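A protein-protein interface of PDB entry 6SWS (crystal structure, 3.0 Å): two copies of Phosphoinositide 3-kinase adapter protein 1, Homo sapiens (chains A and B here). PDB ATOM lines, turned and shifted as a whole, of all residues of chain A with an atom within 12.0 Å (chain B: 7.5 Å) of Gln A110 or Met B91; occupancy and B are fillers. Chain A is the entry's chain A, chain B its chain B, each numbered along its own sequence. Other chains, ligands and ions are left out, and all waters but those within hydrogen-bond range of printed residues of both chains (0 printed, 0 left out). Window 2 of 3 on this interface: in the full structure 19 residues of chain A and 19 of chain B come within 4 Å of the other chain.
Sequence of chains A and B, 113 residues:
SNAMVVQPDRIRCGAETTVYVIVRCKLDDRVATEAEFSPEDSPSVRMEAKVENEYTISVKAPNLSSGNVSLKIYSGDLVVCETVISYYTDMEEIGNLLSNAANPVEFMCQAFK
OE1 of Gln A110 sits close to O of Glu A106 (2.9 Å). The guanidinium group (NH1) of Arg B12 lies within salt-bridge range of the side-chain carboxylate (OD1) of Asp B90, at 2.7 Å.
Among the printed residues, pairs that only touch across the chains: Asn A100 with Arg B12 (3.5 Å), Asp A90 with Leu B97 (3.6 Å), Leu A97 with Glu B93 (3.6 Å), Leu A97 with Arg B12 (3.7 Å), Ile A94 with Ile B94 (3.7 Å), Leu A97 with Ile B94 (3.7 Å), Ile A94 with Leu B97 (3.7 Å), Glu A93 with Leu B97 (3.8 Å), Gln A110 with Met B91 (3.8 Å), Leu A97 with Asp B90 (3.8 Å) and Leu A98 with Ile B94 (3.9 Å).
Gln A110 touches one residue of chain B. Printed residues of chain A within 4 Å of Met B91: Gln A110. No residue of chain A comes within 4 Å of Thr B89. Of chain A, only Leu A97 comes within 4 Å of Asp B90. Ile B94 touches just these residues of chain A: Ile A94 (3.7 Å), Leu A97 (3.7 Å) and Leu A98 (3.9 Å). No residue of chain A comes within 4 Å of Gly B95. Of the printed residues of chain B, Glu A93 touches Leu B97. Of the printed residues of chain A, Leu B97 touches Asp A90, Glu A93 and Ile A94. Of the printed residues of chain A, Arg B12 touches Leu A97 (3.7 Å) and Asn A100 (3.5 Å). Printed residues of chain A within 4 Å of Glu B93: Leu A97. Ala A101 touches none of the printed residues of chain B. Asn B96 touches none of the printed residues of chain A.
Printed residues of chain B that touch a printed residue of chain A: Arg B12, Asp B90, Met B91, Glu B93, Ile B94 and Leu B97. Hydrophobic or aromatic side chains of chain B that line the printed part of chain A: Met B91, Ile B94 and Leu B97. Of the 22 printed residues of chain A, 7 touch a printed residue of chain B. Hydrophobic or aromatic side chains of chain A that line the printed part of chain B: Ile A94, Leu A97 and Leu A98.
Asp A90 touches Leu B97, and with the chains exchanged Leu A97 touches Asp B90. Glu A93 touches Leu B97, and with the chains exchanged Leu A97 touches Glu B93. Ile A94 touches its own counterpart, Ile B94. Ile A94 touches Leu B97, and with the chains exchanged Leu A97 touches Ile B94.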
ATOM      1  N   ASP A  90      20.542  29.484  35.395  1.00  0.00           N
ATOM      2  CA  ASP A  90      20.133  29.831  34.037  1.00  0.00           C
ATOM      3  C   ASP A  90      21.290  29.698  33.054  1.00  0.00           C
ATOM      4  O   ASP A  90      21.145  29.092  31.985  1.00  0.00           O
ATOM      5  CB  ASP A  90      19.571  31.253  34.009  1.00  0.00           C
ATOM      6  CG  ASP A  90      18.428  31.449  34.986  1.00  0.00           C
ATOM      7  OD1 ASP A  90      17.674  30.483  35.221  1.00  0.00           O
ATOM      8  OD2 ASP A  90      18.281  32.573  35.513  1.00  0.00           O
ATOM      9  N   GLU A  93      22.212  26.122  32.144  1.00  0.00           N
ATOM     10  CA  GLU A  93      21.306  25.503  31.186  1.00  0.00           C
ATOM     11  C   GLU A  93      21.474  26.091  29.791  1.00  0.00           C
ATOM     12  O   GLU A  93      21.330  25.371  28.799  1.00  0.00           O
ATOM     13  CB  GLU A  93      19.860  25.638  31.661  1.00  0.00           C
ATOM     14  CG  GLU A  93      18.900  24.681  30.974  1.00  0.00           C
ATOM     15  CD  GLU A  93      19.247  23.228  31.241  1.00  0.00           C
ATOM     16  OE1 GLU A  93      19.805  22.935  32.323  1.00  0.00           O
ATOM     17  OE2 GLU A  93      18.967  22.378  30.372  1.00  0.00           O
ATOM     18  N   ILE A  94      21.763  27.391  29.693  1.00  0.00           N
ATOM     19  CA  ILE A  94      22.079  27.985  28.393  1.00  0.00           C
ATOM     20  C   ILE A  94      23.265  27.267  27.763  1.00  0.00           C
ATOM     21  O   ILE A  94      23.248  26.912  26.577  1.00  0.00           O
ATOM     22  CB  ILE A  94      22.351  29.493  28.540  1.00  0.00           C
ATOM     23  CG1 ILE A  94      21.109  30.214  29.071  1.00  0.00           C
ATOM     24  CG2 ILE A  94      22.810  30.080  27.222  1.00  0.00           C
ATOM     25  CD1 ILE A  94      21.301  31.702  29.230  1.00  0.00           C
ATOM     26  N   GLY A  95      24.312  27.036  28.557  1.00  0.00           N
ATOM     27  CA  GLY A  95      25.468  26.314  28.048  1.00  0.00           C
ATOM     28  C   GLY A  95      25.134  24.889  27.649  1.00  0.00           C
ATOM     29  O   GLY A  95      25.589  24.399  26.610  1.00  0.00           O
ATOM     30  N   ASN A  96      24.336  24.203  28.472  1.00  0.00           N
ATOM     31  CA  ASN A  96      23.945  22.833  28.154  1.00  0.00           C
ATOM     32  C   ASN A  96      23.162  22.772  26.848  1.00  0.00           C
ATOM     33  O   ASN A  96      23.377  21.870  26.030  1.00  0.00           O
ATOM     34  CB  ASN A  96      23.124  22.236  29.297  1.00  0.00           C
ATOM     35  CG  ASN A  96      23.982  21.809  30.468  1.00  0.00           C
ATOM     36  OD1 ASN A  96      23.847  22.330  31.575  1.00  0.00           O
ATOM     37  ND2 ASN A  96      24.875  20.854  30.231  1.00  0.00           N
ATOM     38  N   LEU A  97      22.254  23.726  26.633  1.00  0.00           N
ATOM     39  CA  LEU A  97      21.476  23.741  25.398  1.00  0.00           C
ATOM     40  C   LEU A  97      22.359  24.064  24.200  1.00  0.00           C
ATOM     41  O   LEU A  97      22.183  23.484  23.120  1.00  0.00           O
ATOM     42  CB  LEU A  97      20.316  24.729  25.514  1.00  0.00           C
ATOM     43  CG  LEU A  97      19.227  24.316  26.509  1.00  0.00           C
ATOM     44  CD1 LEU A  97      18.287  25.469  26.821  1.00  0.00           C
ATOM     45  CD2 LEU A  97      18.453  23.121  25.977  1.00  0.00           C
ATOM     46  N   LEU A  98      23.313  24.984  24.365  1.00  0.00           N
ATOM     47  CA  LEU A  98      24.232  25.276  23.272  1.00  0.00           C
ATOM     48  C   LEU A  98      25.093  24.068  22.934  1.00  0.00           C
ATOM     49  O   LEU A  98      25.460  23.872  21.770  1.00  0.00           O
ATOM     50  CB  LEU A  98      25.116  26.472  23.620  1.00  0.00           C
ATOM     51  CG  LEU A  98      24.414  27.826  23.613  1.00  0.00           C
ATOM     52  CD1 LEU A  98      25.267  28.859  24.311  1.00  0.00           C
ATOM     53  CD2 LEU A  98      24.115  28.249  22.185  1.00  0.00           C
ATOM     54  N   SER A  99      25.413  23.242  23.930  1.00  0.00           N
ATOM     55  CA  SER A  99      26.225  22.057  23.682  1.00  0.00           C
ATOM     56  C   SER A  99      25.509  21.001  22.848  1.00  0.00           C
ATOM     57  O   SER A  99      26.145  20.016  22.458  1.00  0.00           O
ATOM     58  CB  SER A  99      26.673  21.444  25.009  1.00  0.00           C
ATOM     59  OG  SER A  99      27.268  22.420  25.846  1.00  0.00           O
ATOM     60  N   ASN A 100      24.220  21.178  22.556  1.00  0.00           N
ATOM     61  CA  ASN A 100      23.462  20.198  21.791  1.00  0.00           C
ATOM     62  C   ASN A 100      23.392  20.508  20.301  1.00  0.00           C
ATOM     63  O   ASN A 100      22.915  19.665  19.534  1.00  0.00           O
ATOM     64  CB  ASN A 100      22.039  20.074  22.348  1.00  0.00           C
ATOM     65  CG  ASN A 100      21.986  19.279  23.636  1.00  0.00           C
ATOM     66  OD1 ASN A 100      22.802  18.384  23.860  1.00  0.00           O
ATOM     67  ND2 ASN A 100      21.020  19.597  24.489  1.00  0.00           N
ATOM     68  N   ALA A 101      23.844  21.684  19.873  1.00  0.00           N
ATOM     69  CA  ALA A 101      23.830  22.013  18.458  1.00  0.00           C
ATOM     70  C   ALA A 101      24.837  21.156  17.696  1.00  0.00           C
ATOM     71  O   ALA A 101      25.787  20.609  18.263  1.00  0.00           O
ATOM     72  CB  ALA A 101      24.131  23.497  18.243  1.00  0.00           C
ATOM     73  N   ALA A 102      24.614  21.041  16.386  1.00  0.00           N
ATOM     74  CA  ALA A 102      25.483  20.212  15.555  1.00  0.00           C
ATOM     75  C   ALA A 102      26.851  20.859  15.381  1.00  0.00           C
ATOM     76  O   ALA A 102      27.873  20.313  15.814  1.00  0.00           O
ATOM     77  CB  ALA A 102      24.825  19.960  14.197  1.00  0.00           C
ATOM     78  N   ASN A 103      26.888  22.025  14.752  1.00  0.00           N
ATOM     79  CA  ASN A 103      28.120  22.740  14.466  1.00  0.00           C
ATOM     80  C   ASN A 103      27.873  24.229  14.677  1.00  0.00           C
ATOM     81  O   ASN A 103      26.723  24.672  14.690  1.00  0.00           O
ATOM     82  CB  ASN A 103      28.603  22.461  13.036  1.00  0.00           C
ATOM     83  CG  ASN A 103      27.723  23.100  11.984  1.00  0.00           C
ATOM     84  OD1 ASN A 103      28.146  24.018  11.287  1.00  0.00           O
ATOM     85  ND2 ASN A 103      26.494  22.614  11.860  1.00  0.00           N
ATOM     86  N   PRO A 104      28.939  25.015  14.864  1.00  0.00           N
ATOM     87  CA  PRO A 104      28.737  26.442  15.182  1.00  0.00           C
ATOM     88  C   PRO A 104      27.999  27.224  14.109  1.00  0.00           C
ATOM     89  O   PRO A 104      27.327  28.212  14.434  1.00  0.00           O
ATOM     90  CB  PRO A 104      30.170  26.956  15.374  1.00  0.00           C
ATOM     91  CG  PRO A 104      30.961  25.753  15.740  1.00  0.00           C
ATOM     92  CD  PRO A 104      30.357  24.629  14.959  1.00  0.00           C
ATOM     93  N   VAL A 105      28.105  26.822  12.839  1.00  0.00           N
ATOM     94  CA  VAL A 105      27.392  27.531  11.781  1.00  0.00           C
ATOM     95  C   VAL A 105      25.881  27.418  11.974  1.00  0.00           C
ATOM     96  O   VAL A 105      25.142  28.365  11.683  1.00  0.00           O
ATOM     97  CB  VAL A 105      27.848  27.016  10.399  1.00  0.00           C
ATOM     98  CG1 VAL A 105      26.847  27.388   9.315  1.00  0.00           C
ATOM     99  CG2 VAL A 105      29.221  27.573  10.058  1.00  0.00           C
ATOM    100  N   GLU A 106      25.400  26.280  12.484  1.00  0.00           N
ATOM    101  CA  GLU A 106      23.978  26.134  12.796  1.00  0.00           C
ATOM    102  C   GLU A 106      23.525  27.177  13.810  1.00  0.00           C
ATOM    103  O   GLU A 106      22.525  27.878  13.600  1.00  0.00           O
ATOM    104  CB  GLU A 106      23.707  24.730  13.336  1.00  0.00           C
ATOM    105  CG  GLU A 106      22.278  24.520  13.805  1.00  0.00           C
ATOM    106  CD  GLU A 106      22.070  23.159  14.438  1.00  0.00           C
ATOM    107  OE1 GLU A 106      23.064  22.578  14.919  1.00  0.00           O
ATOM    108  OE2 GLU A 106      20.920  22.673  14.460  1.00  0.00           O
ATOM    109  N   PHE A 107      24.244  27.274  14.930  1.00  0.00           N
ATOM    110  CA  PHE A 107      23.886  28.226  15.974  1.00  0.00           C
ATOM    111  C   PHE A 107      23.984  29.658  15.466  1.00  0.00           C
ATOM    112  O   PHE A 107      23.163  30.509  15.823  1.00  0.00           O
ATOM    113  CB  PHE A 107      24.784  28.007  17.192  1.00  0.00           C
ATOM    114  CG  PHE A 107      24.916  29.205  18.087  1.00  0.00           C
ATOM    115  CD1 PHE A 107      23.837  29.663  18.829  1.00  0.00           C
ATOM    116  CD2 PHE A 107      26.131  29.860  18.208  1.00  0.00           C
ATOM    117  CE1 PHE A 107      23.967  30.765  19.659  1.00  0.00           C
ATOM    118  CE2 PHE A 107      26.268  30.959  19.034  1.00  0.00           C
ATOM    119  CZ  PHE A 107      25.185  31.412  19.762  1.00  0.00           C
ATOM    120  N   MET A 108      24.967  29.935  14.607  1.00  0.00           N
ATOM    121  CA  MET A 108      25.094  31.279  14.051  1.00  0.00           C
ATOM    122  C   MET A 108      23.928  31.615  13.131  1.00  0.00           C
ATOM    123  O   MET A 108      23.388  32.725  13.191  1.00  0.00           O
ATOM    124  CB  MET A 108      26.420  31.414  13.309  1.00  0.00           C
ATOM    125  CG  MET A 108      27.604  31.441  14.233  1.00  0.00           C
ATOM    126  SD  MET A 108      27.707  32.974  15.170  1.00  0.00           S
ATOM    127  CE  MET A 108      28.415  34.052  13.928  1.00  0.00           C
ATOM    128  N   CYS A 109      23.526  30.672  12.277  1.00  0.00           N
ATOM    129  CA  CYS A 109      22.399  30.920  11.385  1.00  0.00           C
ATOM    130  C   CYS A 109      21.105  31.085  12.171  1.00  0.00           C
ATOM    131  O   CYS A 109      20.239  31.880  11.793  1.00  0.00           O
ATOM    132  CB  CYS A 109      22.269  29.788  10.366  1.00  0.00           C
ATOM    133  SG  CYS A 109      23.599  29.721   9.145  1.00  0.00           S
ATOM    134  N   GLN A 110      20.957  30.344  13.271  1.00  0.00           N
ATOM    135  CA  GLN A 110      19.754  30.495  14.082  1.00  0.00           C
ATOM    136  C   GLN A 110      19.779  31.781  14.899  1.00  0.00           C
ATOM    137  O   GLN A 110      18.719  32.319  15.237  1.00  0.00           O
ATOM    138  CB  GLN A 110      19.576  29.283  14.993  1.00  0.00           C
ATOM    139  CG  GLN A 110      18.925  28.095  14.304  1.00  0.00           C
ATOM    140  CD  GLN A 110      19.564  26.779  14.685  1.00  0.00           C
ATOM    141  OE1 GLN A 110      20.556  26.746  15.413  1.00  0.00           O
ATOM    142  NE2 GLN A 110      18.997  25.683  14.196  1.00  0.00           N
ATOM    143  N   ALA A 111      20.969  32.290  15.222  1.00  0.00           N
ATOM    144  CA  ALA A 111      21.052  33.545  15.959  1.00  0.00           C
ATOM    145  C   ALA A 111      20.848  34.751  15.049  1.00  0.00           C
ATOM    146  O   ALA A 111      20.220  35.735  15.454  1.00  0.00           O
ATOM    147  CB  ALA A 111      22.398  33.640  16.677  1.00  0.00           C
ATOM    148  N   PHE A 112      21.357  34.691  13.819  1.00  0.00           N
ATOM    149  CA  PHE A 112      21.338  35.825  12.906  1.00  0.00           C
ATOM    150  C   PHE A 112      20.181  35.776  11.915  1.00  0.00           C
ATOM    151  O   PHE A 112      20.138  36.592  10.989  1.00  0.00           O
ATOM    152  CB  PHE A 112      22.670  35.915  12.159  1.00  0.00           C
ATOM    153  CG  PHE A 112      23.792  36.445  13.001  1.00  0.00           C
ATOM    154  CD1 PHE A 112      23.966  37.807  13.168  1.00  0.00           C
ATOM    155  CD2 PHE A 112      24.653  35.579  13.652  1.00  0.00           C
ATOM    156  CE1 PHE A 112      24.991  38.295  13.951  1.00  0.00           C
ATOM    157  CE2 PHE A 112      25.676  36.062  14.439  1.00  0.00           C
ATOM    158  CZ  PHE A 112      25.846  37.420  14.588  1.00  0.00           C
ATOM    159  N   LYS A 113      19.245  34.849  12.085  1.00  0.00           N
ATOM    160  CA  LYS A 113      18.068  34.799  11.226  1.00  0.00           C
ATOM    161  C   LYS A 113      16.961  35.680  11.792  1.00  0.00           C
ATOM    162  O   LYS A 113      17.173  36.859  12.075  1.00  0.00           O
ATOM    163  CB  LYS A 113      17.568  33.362  11.067  1.00  0.00           C
ATOM    164  OXT LYS A 113      15.829  35.235  11.980  1.00  0.00           O
ATOM    165  N   ARG B  12      11.001  19.461  25.410  1.00  0.00           N
ATOM    166  CA  ARG B  12      11.980  20.014  24.484  1.00  0.00           C
ATOM    167  C   ARG B  12      11.977  19.226  23.178  1.00  0.00           C
ATOM    168  O   ARG B  12      11.964  17.992  23.187  1.00  0.00           O
ATOM    169  CB  ARG B  12      13.369  19.990  25.121  1.00  0.00           C
ATOM    170  CG  ARG B  12      14.451  20.656  24.294  1.00  0.00           C
ATOM    171  CD  ARG B  12      15.722  20.832  25.108  1.00  0.00           C
ATOM    172  NE  ARG B  12      16.398  19.560  25.341  1.00  0.00           N
ATOM    173  CZ  ARG B  12      17.316  19.045  24.530  1.00  0.00           C
ATOM    174  NH1 ARG B  12      17.666  19.694  23.428  1.00  0.00           N
ATOM    175  NH2 ARG B  12      17.883  17.882  24.820  1.00  0.00           N
ATOM    176  N   TYR B  88       8.921  23.088  22.901  1.00  0.00           N
ATOM    177  CA  TYR B  88       9.799  24.234  22.722  1.00  0.00           C
ATOM    178  C   TYR B  88      11.130  23.759  22.161  1.00  0.00           C
ATOM    179  O   TYR B  88      11.540  22.615  22.380  1.00  0.00           O
ATOM    180  CB  TYR B  88      10.010  24.996  24.036  1.00  0.00           C
ATOM    181  CG  TYR B  88      10.742  24.210  25.100  1.00  0.00           C
ATOM    182  CD1 TYR B  88      10.062  23.338  25.940  1.00  0.00           C
ATOM    183  CD2 TYR B  88      12.111  24.353  25.276  1.00  0.00           C
ATOM    184  CE1 TYR B  88      10.728  22.622  26.917  1.00  0.00           C
ATOM    185  CE2 TYR B  88      12.785  23.642  26.249  1.00  0.00           C
ATOM    186  CZ  TYR B  88      12.089  22.779  27.067  1.00  0.00           C
ATOM    187  OH  TYR B  88      12.758  22.070  28.039  1.00  0.00           O
ATOM    188  N   THR B  89      11.798  24.651  21.438  1.00  0.00           N
ATOM    189  CA  THR B  89      13.098  24.380  20.843  1.00  0.00           C
ATOM    190  C   THR B  89      14.219  24.893  21.739  1.00  0.00           C
ATOM    191  O   THR B  89      14.000  25.682  22.663  1.00  0.00           O
ATOM    192  CB  THR B  89      13.215  25.024  19.460  1.00  0.00           C
ATOM    193  OG1 THR B  89      13.396  26.438  19.608  1.00  0.00           O
ATOM    194  CG2 THR B  89      11.962  24.762  18.643  1.00  0.00           C
ATOM    195  N   ASP B  90      15.434  24.425  21.447  1.00  0.00           N
ATOM    196  CA  ASP B  90      16.605  24.840  22.214  1.00  0.00           C
ATOM    197  C   ASP B  90      16.758  26.356  22.210  1.00  0.00           C
ATOM    198  O   ASP B  90      16.951  26.975  23.263  1.00  0.00           O
ATOM    199  CB  ASP B  90      17.863  24.178  21.649  1.00  0.00           C
ATOM    200  CG  ASP B  90      17.827  22.667  21.761  1.00  0.00           C
ATOM    201  OD1 ASP B  90      17.006  22.151  22.544  1.00  0.00           O
ATOM    202  OD2 ASP B  90      18.622  21.997  21.069  1.00  0.00           O
ATOM    203  N   MET B  91      16.666  26.970  21.028  1.00  0.00           N
ATOM    204  CA  MET B  91      16.863  28.411  20.918  1.00  0.00           C
ATOM    205  C   MET B  91      15.783  29.180  21.671  1.00  0.00           C
ATOM    206  O   MET B  91      16.066  30.207  22.301  1.00  0.00           O
ATOM    207  CB  MET B  91      16.873  28.810  19.442  1.00  0.00           C
ATOM    208  CG  MET B  91      18.004  28.183  18.640  1.00  0.00           C
ATOM    209  SD  MET B  91      19.656  28.603  19.221  1.00  0.00           S
ATOM    210  CE  MET B  91      19.793  30.282  18.618  1.00  0.00           C
ATOM    211  N   GLU B  92      14.544  28.683  21.640  1.00  0.00           N
ATOM    212  CA  GLU B  92      13.462  29.328  22.377  1.00  0.00           C
ATOM    213  C   GLU B  92      13.752  29.342  23.872  1.00  0.00           C
ATOM    214  O   GLU B  92      13.595  30.370  24.544  1.00  0.00           O
ATOM    215  CB  GLU B  92      12.144  28.605  22.102  1.00  0.00           C
ATOM    216  CG  GLU B  92      11.510  28.928  20.763  1.00  0.00           C
ATOM    217  CD  GLU B  92      10.221  28.164  20.539  1.00  0.00           C
ATOM    218  OE1 GLU B  92       9.894  27.874  19.370  1.00  0.00           O
ATOM    219  OE2 GLU B  92       9.538  27.845  21.535  1.00  0.00           O
ATOM    220  N   GLU B  93      14.197  28.204  24.407  1.00  0.00           N
ATOM    221  CA  GLU B  93      14.474  28.133  25.835  1.00  0.00           C
ATOM    222  C   GLU B  93      15.702  28.951  26.207  1.00  0.00           C
ATOM    223  O   GLU B  93      15.740  29.535  27.291  1.00  0.00           O
ATOM    224  CB  GLU B  93      14.630  26.679  26.278  1.00  0.00           C
ATOM    225  CG  GLU B  93      14.935  26.514  27.763  1.00  0.00           C
ATOM    226  CD  GLU B  93      13.694  26.606  28.641  1.00  0.00           C
ATOM    227  OE1 GLU B  93      12.683  27.195  28.203  1.00  0.00           O
ATOM    228  OE2 GLU B  93      13.729  26.084  29.774  1.00  0.00           O
ATOM    229  N   ILE B  94      16.713  29.000  25.336  1.00  0.00           N
ATOM    230  CA  ILE B  94      17.863  29.860  25.605  1.00  0.00           C
ATOM    231  C   ILE B  94      17.431  31.319  25.660  1.00  0.00           C
ATOM    232  O   ILE B  94      17.880  32.084  26.523  1.00  0.00           O
ATOM    233  CB  ILE B  94      18.970  29.641  24.556  1.00  0.00           C
ATOM    234  CG1 ILE B  94      19.488  28.205  24.616  1.00  0.00           C
ATOM    235  CG2 ILE B  94      20.115  30.612  24.786  1.00  0.00           C
ATOM    236  CD1 ILE B  94      20.502  27.885  23.536  1.00  0.00           C
ATOM    237  N   GLY B  95      16.551  31.731  24.743  1.00  0.00           N
ATOM    238  CA  GLY B  95      16.060  33.098  24.774  1.00  0.00           C
ATOM    239  C   GLY B  95      15.260  33.400  26.027  1.00  0.00           C
ATOM    240  O   GLY B  95      15.397  34.473  26.621  1.00  0.00           O
ATOM    241  N   ASN B  96      14.430  32.447  26.461  1.00  0.00           N
ATOM    242  CA  ASN B  96      13.677  32.644  27.698  1.00  0.00           C
ATOM    243  C   ASN B  96      14.601  32.693  28.910  1.00  0.00           C
ATOM    244  O   ASN B  96      14.397  33.501  29.825  1.00  0.00           O
ATOM    245  CB  ASN B  96      12.637  31.537  27.865  1.00  0.00           C
ATOM    246  CG  ASN B  96      11.478  31.676  26.902  1.00  0.00           C
ATOM    247  OD1 ASN B  96      10.374  32.050  27.293  1.00  0.00           O
ATOM    248  ND2 ASN B  96      11.725  31.377  25.632  1.00  0.00           N
ATOM    249  N   LEU B  97      15.633  31.848  28.927  1.00  0.00           N
ATOM    250  CA  LEU B  97      16.580  31.847  30.033  1.00  0.00           C
ATOM    251  C   LEU B  97      17.402  33.126  30.067  1.00  0.00           C
ATOM    252  O   LEU B  97      17.789  33.579  31.146  1.00  0.00           O
ATOM    253  CB  LEU B  97      17.488  30.621  29.942  1.00  0.00           C
ATOM    254  CG  LEU B  97      16.845  29.319  30.423  1.00  0.00           C
ATOM    255  CD1 LEU B  97      17.634  28.117  29.932  1.00  0.00           C
ATOM    256  CD2 LEU B  97      16.722  29.304  31.940  1.00  0.00           C
